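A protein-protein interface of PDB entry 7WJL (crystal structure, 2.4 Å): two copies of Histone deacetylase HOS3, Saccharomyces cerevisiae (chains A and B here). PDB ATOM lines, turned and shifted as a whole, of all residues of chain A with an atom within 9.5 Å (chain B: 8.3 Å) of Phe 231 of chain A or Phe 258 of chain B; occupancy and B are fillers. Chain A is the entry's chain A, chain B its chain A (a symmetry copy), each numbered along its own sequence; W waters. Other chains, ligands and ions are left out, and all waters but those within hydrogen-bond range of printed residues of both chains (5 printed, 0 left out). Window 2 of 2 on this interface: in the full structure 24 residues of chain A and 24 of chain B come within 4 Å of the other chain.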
ATOM      1  N   TRP A 212     -29.554   6.957  16.590  1.00  0.00           N
ATOM      2  CA  TRP A 212     -28.757   7.013  17.811  1.00  0.00           C
ATOM      3  C   TRP A 212     -28.658   5.638  18.458  1.00  0.00           C
ATOM      4  O   TRP A 212     -27.595   5.263  18.966  1.00  0.00           O
ATOM      5  CB  TRP A 212     -29.344   8.035  18.797  1.00  0.00           C
ATOM      6  CG  TRP A 212     -28.956   9.451  18.503  1.00  0.00           C
ATOM      7  CD1 TRP A 212     -29.655  10.347  17.751  1.00  0.00           C
ATOM      8  CD2 TRP A 212     -27.785  10.141  18.960  1.00  0.00           C
ATOM      9  NE1 TRP A 212     -28.998  11.546  17.710  1.00  0.00           N
ATOM     10  CE2 TRP A 212     -27.847  11.453  18.449  1.00  0.00           C
ATOM     11  CE3 TRP A 212     -26.696   9.781  19.763  1.00  0.00           C
ATOM     12  CZ2 TRP A 212     -26.859  12.410  18.706  1.00  0.00           C
ATOM     13  CZ3 TRP A 212     -25.710  10.737  20.015  1.00  0.00           C
ATOM     14  CH2 TRP A 212     -25.804  12.036  19.486  1.00  0.00           C
ATOM     15  N   ALA A 215     -26.100   3.651  16.603  1.00  0.00           N
ATOM     16  CA  ALA A 215     -24.739   4.058  16.943  1.00  0.00           C
ATOM     17  C   ALA A 215     -24.249   3.435  18.244  1.00  0.00           C
ATOM     18  O   ALA A 215     -23.052   3.510  18.532  1.00  0.00           O
ATOM     19  CB  ALA A 215     -24.639   5.584  17.046  1.00  0.00           C
ATOM     20  N   GLY A 216     -25.131   2.816  19.019  1.00  0.00           N
ATOM     21  CA  GLY A 216     -24.755   2.236  20.287  1.00  0.00           C
ATOM     22  C   GLY A 216     -25.073   3.061  21.516  1.00  0.00           C
ATOM     23  O   GLY A 216     -24.657   2.676  22.618  1.00  0.00           O
ATOM     24  N   PHE A 217     -25.790   4.176  21.380  1.00  0.00           N
ATOM     25  CA  PHE A 217     -26.156   4.963  22.552  1.00  0.00           C
ATOM     26  C   PHE A 217     -27.469   4.457  23.139  1.00  0.00           C
ATOM     27  O   PHE A 217     -28.379   4.037  22.406  1.00  0.00           O
ATOM     28  CB  PHE A 217     -26.276   6.451  22.213  1.00  0.00           C
ATOM     29  CG  PHE A 217     -24.970   7.106  21.866  1.00  0.00           C
ATOM     30  CD1 PHE A 217     -24.169   7.644  22.853  1.00  0.00           C
ATOM     31  CD2 PHE A 217     -24.554   7.195  20.542  1.00  0.00           C
ATOM     32  CE1 PHE A 217     -22.966   8.260  22.533  1.00  0.00           C
ATOM     33  CE2 PHE A 217     -23.357   7.807  20.213  1.00  0.00           C
ATOM     34  CZ  PHE A 217     -22.557   8.340  21.208  1.00  0.00           C
ATOM     35  N   LYS A 218     -27.559   4.509  24.459  1.00  0.00           N
ATOM     36  CA  LYS A 218     -28.705   3.952  25.167  1.00  0.00           C
ATOM     37  C   LYS A 218     -29.962   4.753  24.854  1.00  0.00           C
ATOM     38  O   LYS A 218     -29.956   5.978  24.999  1.00  0.00           O
ATOM     39  CB  LYS A 218     -28.448   3.962  26.680  1.00  0.00           C
ATOM     40  CG  LYS A 218     -29.531   3.241  27.499  1.00  0.00           C
ATOM     41  CD  LYS A 218     -29.345   3.434  29.009  1.00  0.00           C
ATOM     42  CE  LYS A 218     -29.994   4.716  29.473  1.00  0.00           C
ATOM     43  NZ  LYS A 218     -31.477   4.625  29.470  1.00  0.00           N
ATOM     44  N   ASP A 225     -28.284  -0.162  31.706  1.00  0.00           N
ATOM     45  CA  ASP A 225     -27.772  -1.519  31.692  1.00  0.00           C
ATOM     46  C   ASP A 225     -26.249  -1.488  31.745  1.00  0.00           C
ATOM     47  O   ASP A 225     -25.617  -0.537  31.275  1.00  0.00           O
ATOM     48  CB  ASP A 225     -28.254  -2.246  30.423  1.00  0.00           C
ATOM     49  CG  ASP A 225     -27.884  -3.710  30.410  1.00  0.00           C
ATOM     50  OD1 ASP A 225     -27.486  -4.237  31.477  1.00  0.00           O
ATOM     51  OD2 ASP A 225     -27.989  -4.328  29.329  1.00  0.00           O
ATOM     52  N   SER A 227     -24.512  -3.116  29.940  1.00  0.00           N
ATOM     53  CA  SER A 227     -24.110  -3.219  28.544  1.00  0.00           C
ATOM     54  C   SER A 227     -23.438  -1.942  28.029  1.00  0.00           C
ATOM     55  O   SER A 227     -22.643  -2.010  27.084  1.00  0.00           O
ATOM     56  CB  SER A 227     -25.348  -3.571  27.711  1.00  0.00           C
ATOM     57  OG  SER A 227     -25.242  -3.112  26.378  1.00  0.00           O
ATOM     58  N   TYR A 228     -23.718  -0.793  28.638  1.00  0.00           N
ATOM     59  CA  TYR A 228     -23.200   0.494  28.187  1.00  0.00           C
ATOM     60  C   TYR A 228     -22.070   0.955  29.089  1.00  0.00           C
ATOM     61  O   TYR A 228     -22.106   0.724  30.298  1.00  0.00           O
ATOM     62  CB  TYR A 228     -24.303   1.549  28.184  1.00  0.00           C
ATOM     63  CG  TYR A 228     -25.438   1.195  27.265  1.00  0.00           C
ATOM     64  CD1 TYR A 228     -25.405   1.560  25.922  1.00  0.00           C
ATOM     65  CD2 TYR A 228     -26.538   0.481  27.726  1.00  0.00           C
ATOM     66  CE1 TYR A 228     -26.443   1.242  25.066  1.00  0.00           C
ATOM     67  CE2 TYR A 228     -27.582   0.149  26.873  1.00  0.00           C
ATOM     68  CZ  TYR A 228     -27.530   0.532  25.542  1.00  0.00           C
ATOM     69  OH  TYR A 228     -28.561   0.216  24.675  1.00  0.00           O
ATOM     70  N   ASP A 229     -21.080   1.621  28.498  1.00  0.00           N
ATOM     71  CA  ASP A 229     -19.974   2.183  29.258  1.00  0.00           C
ATOM     72  C   ASP A 229     -20.438   3.424  30.023  1.00  0.00           C
ATOM     73  O   ASP A 229     -21.625   3.759  30.058  1.00  0.00           O
ATOM     74  CB  ASP A 229     -18.797   2.490  28.332  1.00  0.00           C
ATOM     75  CG  ASP A 229     -19.112   3.570  27.290  1.00  0.00           C
ATOM     76  OD1 ASP A 229     -20.082   4.351  27.445  1.00  0.00           O
ATOM     77  OD2 ASP A 229     -18.375   3.626  26.292  1.00  0.00           O
ATOM     78  N   ASP A 230     -19.480   4.106  30.660  1.00  0.00           N
ATOM     79  CA  ASP A 230     -19.791   5.266  31.494  1.00  0.00           C
ATOM     80  C   ASP A 230     -20.335   6.439  30.701  1.00  0.00           C
ATOM     81  O   ASP A 230     -20.795   7.417  31.305  1.00  0.00           O
ATOM     82  CB  ASP A 230     -18.553   5.729  32.254  1.00  0.00           C
ATOM     83  CG  ASP A 230     -18.115   4.740  33.299  1.00  0.00           C
ATOM     84  OD1 ASP A 230     -18.934   3.869  33.665  1.00  0.00           O
ATOM     85  OD2 ASP A 230     -16.954   4.838  33.752  1.00  0.00           O
ATOM     86  N   PHE A 231     -20.287   6.373  29.376  1.00  0.00           N
ATOM     87  CA  PHE A 231     -20.791   7.425  28.516  1.00  0.00           C
ATOM     88  C   PHE A 231     -22.075   7.002  27.835  1.00  0.00           C
ATOM     89  O   PHE A 231     -22.523   7.659  26.889  1.00  0.00           O
ATOM     90  CB  PHE A 231     -19.704   7.817  27.513  1.00  0.00           C
ATOM     91  CG  PHE A 231     -18.395   8.159  28.182  1.00  0.00           C
ATOM     92  CD1 PHE A 231     -18.224   9.391  28.804  1.00  0.00           C
ATOM     93  CD2 PHE A 231     -17.364   7.231  28.259  1.00  0.00           C
ATOM     94  CE1 PHE A 231     -17.033   9.710  29.458  1.00  0.00           C
ATOM     95  CE2 PHE A 231     -16.165   7.545  28.914  1.00  0.00           C
ATOM     96  CZ  PHE A 231     -16.003   8.787  29.512  1.00  0.00           C
ATOM     97  N   GLY A 232     -22.680   5.914  28.304  1.00  0.00           N
ATOM     98  CA  GLY A 232     -23.907   5.427  27.707  1.00  0.00           C
ATOM     99  C   GLY A 232     -23.739   4.931  26.292  1.00  0.00           C
ATOM    100  O   GLY A 232     -24.685   5.004  25.500  1.00  0.00           O
ATOM    101  N   LYS A 233     -22.555   4.421  25.951  1.00  0.00           N
ATOM    102  CA  LYS A 233     -22.267   3.939  24.610  1.00  0.00           C
ATOM    103  C   LYS A 233     -21.822   2.482  24.628  1.00  0.00           C
ATOM    104  O   LYS A 233     -21.199   2.013  25.580  1.00  0.00           O
ATOM    105  CB  LYS A 233     -21.176   4.783  23.926  1.00  0.00           C
ATOM    106  CG  LYS A 233     -20.985   4.362  22.494  1.00  0.00           C
ATOM    107  CD  LYS A 233     -20.746   5.505  21.557  1.00  0.00           C
ATOM    108  CE  LYS A 233     -21.005   5.058  20.120  1.00  0.00           C
ATOM    109  NZ  LYS A 233     -20.423   3.703  19.808  1.00  0.00           N
ATOM    110  N   LYS A 234     -22.148   1.777  23.552  1.00  0.00           N
ATOM    111  CA  LYS A 234     -21.576   0.475  23.262  1.00  0.00           C
ATOM    112  C   LYS A 234     -21.316   0.387  21.759  1.00  0.00           C
ATOM    113  O   LYS A 234     -21.652   1.295  20.993  1.00  0.00           O
ATOM    114  CB  LYS A 234     -22.493  -0.652  23.749  1.00  0.00           C
ATOM    115  CG  LYS A 234     -23.847  -0.697  23.061  1.00  0.00           C
ATOM    116  CD  LYS A 234     -24.704  -1.798  23.666  1.00  0.00           C
ATOM    117  CE  LYS A 234     -26.096  -1.849  23.028  1.00  0.00           C
ATOM    118  NZ  LYS A 234     -26.999  -2.708  23.867  1.00  0.00           N
ATOM    119  N   HIS A 275     -18.320   9.366  16.219  1.00  0.00           N
ATOM    120  CA  HIS A 275     -19.086   8.717  17.290  1.00  0.00           C
ATOM    121  C   HIS A 275     -20.124   7.739  16.752  1.00  0.00           C
ATOM    122  O   HIS A 275     -21.171   7.536  17.372  1.00  0.00           O
ATOM    123  CB  HIS A 275     -19.753   9.757  18.185  1.00  0.00           C
ATOM    124  CG  HIS A 275     -18.823  10.842  18.615  1.00  0.00           C
ATOM    125  ND1 HIS A 275     -17.853  10.648  19.576  1.00  0.00           N
ATOM    126  CD2 HIS A 275     -18.676  12.114  18.182  1.00  0.00           C
ATOM    127  CE1 HIS A 275     -17.167  11.766  19.738  1.00  0.00           C
ATOM    128  NE2 HIS A 275     -17.644  12.668  18.899  1.00  0.00           N
ATOM    129  N   ASN B 250     -14.203  15.336  17.438  1.00  0.00           N
ATOM    130  CA  ASN B 250     -13.667  14.175  18.132  1.00  0.00           C
ATOM    131  C   ASN B 250     -12.766  14.540  19.310  1.00  0.00           C
ATOM    132  O   ASN B 250     -12.158  13.640  19.913  1.00  0.00           O
ATOM    133  CB  ASN B 250     -12.930  13.286  17.140  1.00  0.00           C
ATOM    134  CG  ASN B 250     -13.877  12.654  16.151  1.00  0.00           C
ATOM    135  OD1 ASN B 250     -14.782  11.910  16.532  1.00  0.00           O
ATOM    136  ND2 ASN B 250     -13.701  12.970  14.884  1.00  0.00           N
ATOM    137  N   SER B 251     -12.685  15.828  19.663  1.00  0.00           N
ATOM    138  CA  SER B 251     -11.947  16.321  20.817  1.00  0.00           C
ATOM    139  C   SER B 251     -12.903  16.791  21.910  1.00  0.00           C
ATOM    140  O   SER B 251     -14.120  16.910  21.711  1.00  0.00           O
ATOM    141  CB  SER B 251     -11.017  17.480  20.421  1.00  0.00           C
ATOM    142  OG  SER B 251      -9.919  17.016  19.655  1.00  0.00           O
ATOM    143  N   PHE B 252     -12.314  17.074  23.070  1.00  0.00           N
ATOM    144  CA  PHE B 252     -13.054  17.577  24.214  1.00  0.00           C
ATOM    145  C   PHE B 252     -13.924  18.761  23.784  1.00  0.00           C
ATOM    146  O   PHE B 252     -13.500  19.566  22.952  1.00  0.00           O
ATOM    147  CB  PHE B 252     -12.065  17.986  25.318  1.00  0.00           C
ATOM    148  CG  PHE B 252     -12.700  18.672  26.495  1.00  0.00           C
ATOM    149  CD1 PHE B 252     -12.945  20.035  26.471  1.00  0.00           C
ATOM    150  CD2 PHE B 252     -13.058  17.944  27.627  1.00  0.00           C
ATOM    151  CE1 PHE B 252     -13.547  20.667  27.553  1.00  0.00           C
ATOM    152  CE2 PHE B 252     -13.655  18.571  28.717  1.00  0.00           C
ATOM    153  CZ  PHE B 252     -13.900  19.930  28.677  1.00  0.00           C
ATOM    154  N   PRO B 253     -15.135  18.906  24.323  1.00  0.00           N
ATOM    155  CA  PRO B 253     -15.835  18.072  25.305  1.00  0.00           C
ATOM    156  C   PRO B 253     -16.481  16.784  24.740  1.00  0.00           C
ATOM    157  O   PRO B 253     -17.231  16.131  25.473  1.00  0.00           O
ATOM    158  CB  PRO B 253     -16.917  19.015  25.842  1.00  0.00           C
ATOM    159  CG  PRO B 253     -17.227  19.923  24.672  1.00  0.00           C
ATOM    160  CD  PRO B 253     -15.898  20.124  23.977  1.00  0.00           C
ATOM    161  N   THR B 254     -16.191  16.399  23.496  1.00  0.00           N
ATOM    162  CA  THR B 254     -16.740  15.162  22.915  1.00  0.00           C
ATOM    163  C   THR B 254     -15.627  14.294  22.342  1.00  0.00           C
ATOM    164  O   THR B 254     -15.668  13.849  21.192  1.00  0.00           O
ATOM    165  CB  THR B 254     -17.794  15.464  21.840  1.00  0.00           C
ATOM    166  OG1 THR B 254     -17.215  16.257  20.784  1.00  0.00           O
ATOM    167  CG2 THR B 254     -18.981  16.214  22.453  1.00  0.00           C
ATOM    168  N   GLU B 255     -14.616  14.020  23.159  1.00  0.00           N
ATOM    169  CA  GLU B 255     -13.487  13.236  22.689  1.00  0.00           C
ATOM    170  C   GLU B 255     -13.945  11.850  22.251  1.00  0.00           C
ATOM    171  O   GLU B 255     -14.768  11.202  22.907  1.00  0.00           O
ATOM    172  CB  GLU B 255     -12.415  13.126  23.773  1.00  0.00           C
ATOM    173  CG  GLU B 255     -11.062  12.638  23.242  1.00  0.00           C
ATOM    174  CD  GLU B 255     -10.189  12.027  24.323  1.00  0.00           C
ATOM    175  OE1 GLU B 255     -10.619  12.002  25.497  1.00  0.00           O
ATOM    176  OE2 GLU B 255      -9.073  11.567  24.001  1.00  0.00           O
ATOM    177  N   SER B 256     -13.400  11.403  21.128  1.00  0.00           N
ATOM    178  CA  SER B 256     -13.768  10.109  20.580  1.00  0.00           C
ATOM    179  C   SER B 256     -13.524   9.007  21.609  1.00  0.00           C
ATOM    180  O   SER B 256     -12.400   8.827  22.086  1.00  0.00           O
ATOM    181  CB  SER B 256     -12.970   9.858  19.304  1.00  0.00           C
ATOM    182  OG  SER B 256     -13.580   8.836  18.543  1.00  0.00           O
ATOM    183  N   GLY B 257     -14.581   8.269  21.951  1.00  0.00           N
ATOM    184  CA  GLY B 257     -14.528   7.240  22.970  1.00  0.00           C
ATOM    185  C   GLY B 257     -15.017   7.672  24.339  1.00  0.00           C
ATOM    186  O   GLY B 257     -15.309   6.811  25.171  1.00  0.00           O
ATOM    187  N   PHE B 258     -15.153   8.974  24.579  1.00  0.00           N
ATOM    188  CA  PHE B 258     -15.412   9.529  25.903  1.00  0.00           C
ATOM    189  C   PHE B 258     -16.451  10.638  25.808  1.00  0.00           C
ATOM    190  O   PHE B 258     -16.257  11.745  26.308  1.00  0.00           O
ATOM    191  CB  PHE B 258     -14.109  10.057  26.518  1.00  0.00           C
ATOM    192  CG  PHE B 258     -13.008   9.028  26.565  1.00  0.00           C
ATOM    193  CD1 PHE B 258     -12.997   8.050  27.552  1.00  0.00           C
ATOM    194  CD2 PHE B 258     -12.001   9.021  25.607  1.00  0.00           C
ATOM    195  CE1 PHE B 258     -11.989   7.084  27.591  1.00  0.00           C
ATOM    196  CE2 PHE B 258     -10.987   8.055  25.638  1.00  0.00           C
ATOM    197  CZ  PHE B 258     -10.983   7.084  26.628  1.00  0.00           C
ATOM    198  N   ALA B 259     -17.574  10.354  25.157  1.00  0.00           N
ATOM    199  CA  ALA B 259     -18.466  11.414  24.707  1.00  0.00           C
ATOM    200  C   ALA B 259     -19.918  11.026  24.947  1.00  0.00           C
ATOM    201  O   ALA B 259     -20.314   9.884  24.705  1.00  0.00           O
ATOM    202  CB  ALA B 259     -18.233  11.714  23.218  1.00  0.00           C
ATOM    203  N   THR B 260     -20.708  11.983  25.420  1.00  0.00           N
ATOM    204  CA  THR B 260     -22.108  11.714  25.698  1.00  0.00           C
ATOM    205  C   THR B 260     -22.981  12.229  24.566  1.00  0.00           C
ATOM    206  O   THR B 260     -22.658  13.222  23.899  1.00  0.00           O
ATOM    207  CB  THR B 260     -22.565  12.342  27.014  1.00  0.00           C
ATOM    208  OG1 THR B 260     -22.494  13.769  26.912  1.00  0.00           O
ATOM    209  CG2 THR B 260     -21.700  11.877  28.151  1.00  0.00           C
ATOM    210  N   LYS B 261     -24.084  11.505  24.351  1.00  0.00           N
ATOM    211  CA  LYS B 261     -25.179  11.913  23.482  1.00  0.00           C
ATOM    212  C   LYS B 261     -25.404  13.420  23.574  1.00  0.00           C
ATOM    213  O   LYS B 261     -25.364  14.144  22.570  1.00  0.00           O
ATOM    214  CB  LYS B 261     -26.435  11.101  23.888  1.00  0.00           C
ATOM    215  CG  LYS B 261     -27.758  11.416  23.187  1.00  0.00           C
ATOM    216  CD  LYS B 261     -28.963  10.544  23.708  1.00  0.00           C
ATOM    217  CE  LYS B 261     -29.110   9.198  22.955  1.00  0.00           C
ATOM    218  NZ  LYS B 261     -30.345   8.334  23.224  1.00  0.00           N
ATOM    219  N   GLU B 262     -25.585  13.913  24.795  1.00  0.00           N
ATOM    220  CA  GLU B 262     -25.988  15.300  24.965  1.00  0.00           C
ATOM    221  C   GLU B 262     -24.904  16.260  24.476  1.00  0.00           C
ATOM    222  O   GLU B 262     -25.204  17.266  23.823  1.00  0.00           O
ATOM    223  CB  GLU B 262     -26.344  15.571  26.431  1.00  0.00           C
ATOM    224  CG  GLU B 262     -26.916  16.966  26.682  1.00  0.00           C
ATOM    225  CD  GLU B 262     -28.037  17.364  25.704  1.00  0.00           C
ATOM    226  OE1 GLU B 262     -28.977  16.557  25.467  1.00  0.00           O
ATOM    227  OE2 GLU B 262     -27.976  18.496  25.175  1.00  0.00           O
ATOM    228  N   ASN B 263     -23.640  15.965  24.769  1.00  0.00           N
ATOM    229  CA  ASN B 263     -22.584  16.878  24.335  1.00  0.00           C
ATOM    230  C   ASN B 263     -22.325  16.772  22.839  1.00  0.00           C
ATOM    231  O   ASN B 263     -21.979  17.778  22.202  1.00  0.00           O
ATOM    232  CB  ASN B 263     -21.308  16.616  25.134  1.00  0.00           C
ATOM    233  CG  ASN B 263     -21.450  17.047  26.584  1.00  0.00           C
ATOM    234  OD1 ASN B 263     -22.236  17.939  26.897  1.00  0.00           O
ATOM    235  ND2 ASN B 263     -20.701  16.412  27.471  1.00  0.00           N
ATOM    236  N   ILE B 264     -22.484  15.575  22.266  1.00  0.00           N
ATOM    237  CA  ILE B 264     -22.376  15.428  20.822  1.00  0.00           C
ATOM    238  C   ILE B 264     -23.443  16.273  20.134  1.00  0.00           C
ATOM    239  O   ILE B 264     -23.158  16.968  19.155  1.00  0.00           O
ATOM    240  CB  ILE B 264     -22.469  13.939  20.422  1.00  0.00           C
ATOM    241  CG1 ILE B 264     -21.259  13.153  20.961  1.00  0.00           C
ATOM    242  CG2 ILE B 264     -22.564  13.792  18.922  1.00  0.00           C
ATOM    243  CD1 ILE B 264     -21.467  11.643  21.032  1.00  0.00           C
ATOM    244  N   HIS B 349      -5.131  14.658  16.845  1.00  0.00           N
ATOM    245  CA  HIS B 349      -6.157  14.145  15.938  1.00  0.00           C
ATOM    246  C   HIS B 349      -5.982  14.628  14.478  1.00  0.00           C
ATOM    247  O   HIS B 349      -6.831  14.336  13.630  1.00  0.00           O
ATOM    248  CB  HIS B 349      -7.562  14.537  16.433  1.00  0.00           C
ATOM    249  CG  HIS B 349      -8.243  13.496  17.274  1.00  0.00           C
ATOM    250  ND1 HIS B 349      -8.513  13.682  18.613  1.00  0.00           N
ATOM    251  CD2 HIS B 349      -8.729  12.269  16.961  1.00  0.00           C
ATOM    252  CE1 HIS B 349      -9.125  12.613  19.094  1.00  0.00           C
ATOM    253  NE2 HIS B 349      -9.267  11.740  18.111  1.00  0.00           N
HETATM  254  O   HOH W   1     -15.341   9.510  16.378  1.00  0.00           O
HETATM  255  O   HOH W   2     -30.087   6.107  21.630  1.00  0.00           O
HETATM  256  O   HOH W   3     -24.539   9.400  26.213  1.00  0.00           O
HETATM  257  O   HOH W   4     -17.390   8.401  21.503  1.00  0.00           O
HETATM  258  O   HOH W   5     -17.532   5.605  24.724  1.00  0.00           O
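NZ of Lys 261 of chain B is in hydrogen-bond range of O of Lys 218 of chain A (3.0 Å). A ring nitrogen (NE2) of His 275 of chain A sits close to the backbone carbonyl oxygen (O) of Thr 254 of chain B (3.2 Å).
The backbone carbonyl oxygen of Trp 212 of chain A is in hydrogen-bond range of the backbone NH of Phe 217 of chain A, at 3.2 Å. The backbone carbonyl oxygen (O) of Gly 232 of chain A sits at hydrogen-bond distance from the backbone NH (N) of Lys 218 of chain A (3.1 Å). OD1 of Asp 229 of chain A is in hydrogen-bond range of N of Phe 231 of chain A (2.8 Å). The backbone NH (N) of Ser 256 of chain B lies within hydrogen-bond range of the backbone carbonyl oxygen (O) of Asn 250 of chain B (2.8 Å). O of Ser 251 of chain B lies close to OG1 of Thr 254 of chain B.
CZ3 of Trp 212 of chain A touches CA of Lys 261 of chain B (3.7 Å). Trp 212 of chain A touches Ile 264 of chain B. CE1 of Phe 217 of chain A touches O of Ala 259 of chain B, 3.8 Å away. Lys 261 of chain B touches Phe 217 of chain A (N to CE1, 3.9 Å). O of Gly 257 of chain B touches CD2 of Phe 231 of chain A (3.7 Å). Phe 231 of chain A touches Phe 258 of chain B (CE2 to CD1, 3.5 Å). CB of Phe 231 of chain A touches O of Ala 259 of chain B, at 3.5 Å. His 275 of chain A touches Ser 256 of chain B (CE1 to CA, 3.9 Å). CE1 of His 275 of chain A touches CB of Ala 259 of chain B (3.6 Å). CD1 of Ile 264 of chain B touches CG of His 275 of chain A (3.7 Å).
Of the printed residues of chain B, Trp 212 of chain A touches Lys 261 (3.7 Å) and Ile 264 (3.7 Å). Of the printed residues of chain B, Phe 217 of chain A touches Ala 259 (3.8 Å), Lys 261 (3.9 Å) and Ile 264 (3.5 Å). Tyr 228 of chain A touches none of the printed residues of chain B. Printed residues of chain B within 4 Å of Phe 231 of chain A: Gly 257 (3.7 Å), Phe 258 (3.5 Å) and Ala 259 (3.5 Å). Of chain A, only Phe 231 (3.7 Å) comes within 4 Å of Gly 257 of chain B. Phe 258 of chain B touches just one residue of chain A: Phe 231 (3.5 Å). Ala 259 of chain B touches just these residues of chain A: Phe 217 (3.8 Å), Phe 231 (3.5 Å) and His 275 (3.6 Å). The nearest residue of chain A that does not touch Phe 258 of chain B is His 275 of chain A (5.9 Å). The nearest printed residue of chain A that does not touch Ser 256 of chain B is Phe 231 of chain A (7.9 Å).
Along chain A the printed residues that touch a printed residue of chain B span positions 212 to 275. Printed residues of chain B that touch a printed residue of chain A: Asn 250, Thr 254, Ser 256, Gly 257, Phe 258, Ala 259, Lys 261 and Ile 264. Among the printed residues, no Asp or Glu carboxylate lies within 4 Å of a Lys or Arg side-chain nitrogen of the other chain.
No position is printed for both chains. Of the 14 pairs that touch across the chains among the printed residues, none has its exchanged pair printed and touching as well.
Water W1 lies within hydrogen-bond range of the side-chain amide oxygen of Asn 250 of chain B, the side-chain hydroxyl of Ser 256 of chain B and the backbone NH of His 275 of chain A. Water W5 bridges O of Gly 257 of chain B (2.6 Å) and OD2 of Asp 229 of chain A (2.7 Å). Water W3 lies within hydrogen-bond range of O of Phe 231 of chain A and N of Lys 261 of chain B. Water W2 lies within hydrogen-bond range of NZ of Lys 261 of chain B (2.8 Å), O of Phe 217 of chain A (2.8 Å) and O of Lys 218 of chain A (3.4 Å). Water W4 lies within hydrogen-bond range of the backbone NH of Gly 257 of chain B (2.8 Å) and a ring nitrogen (ND1) of His 275 of chain A (3.0 Å).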
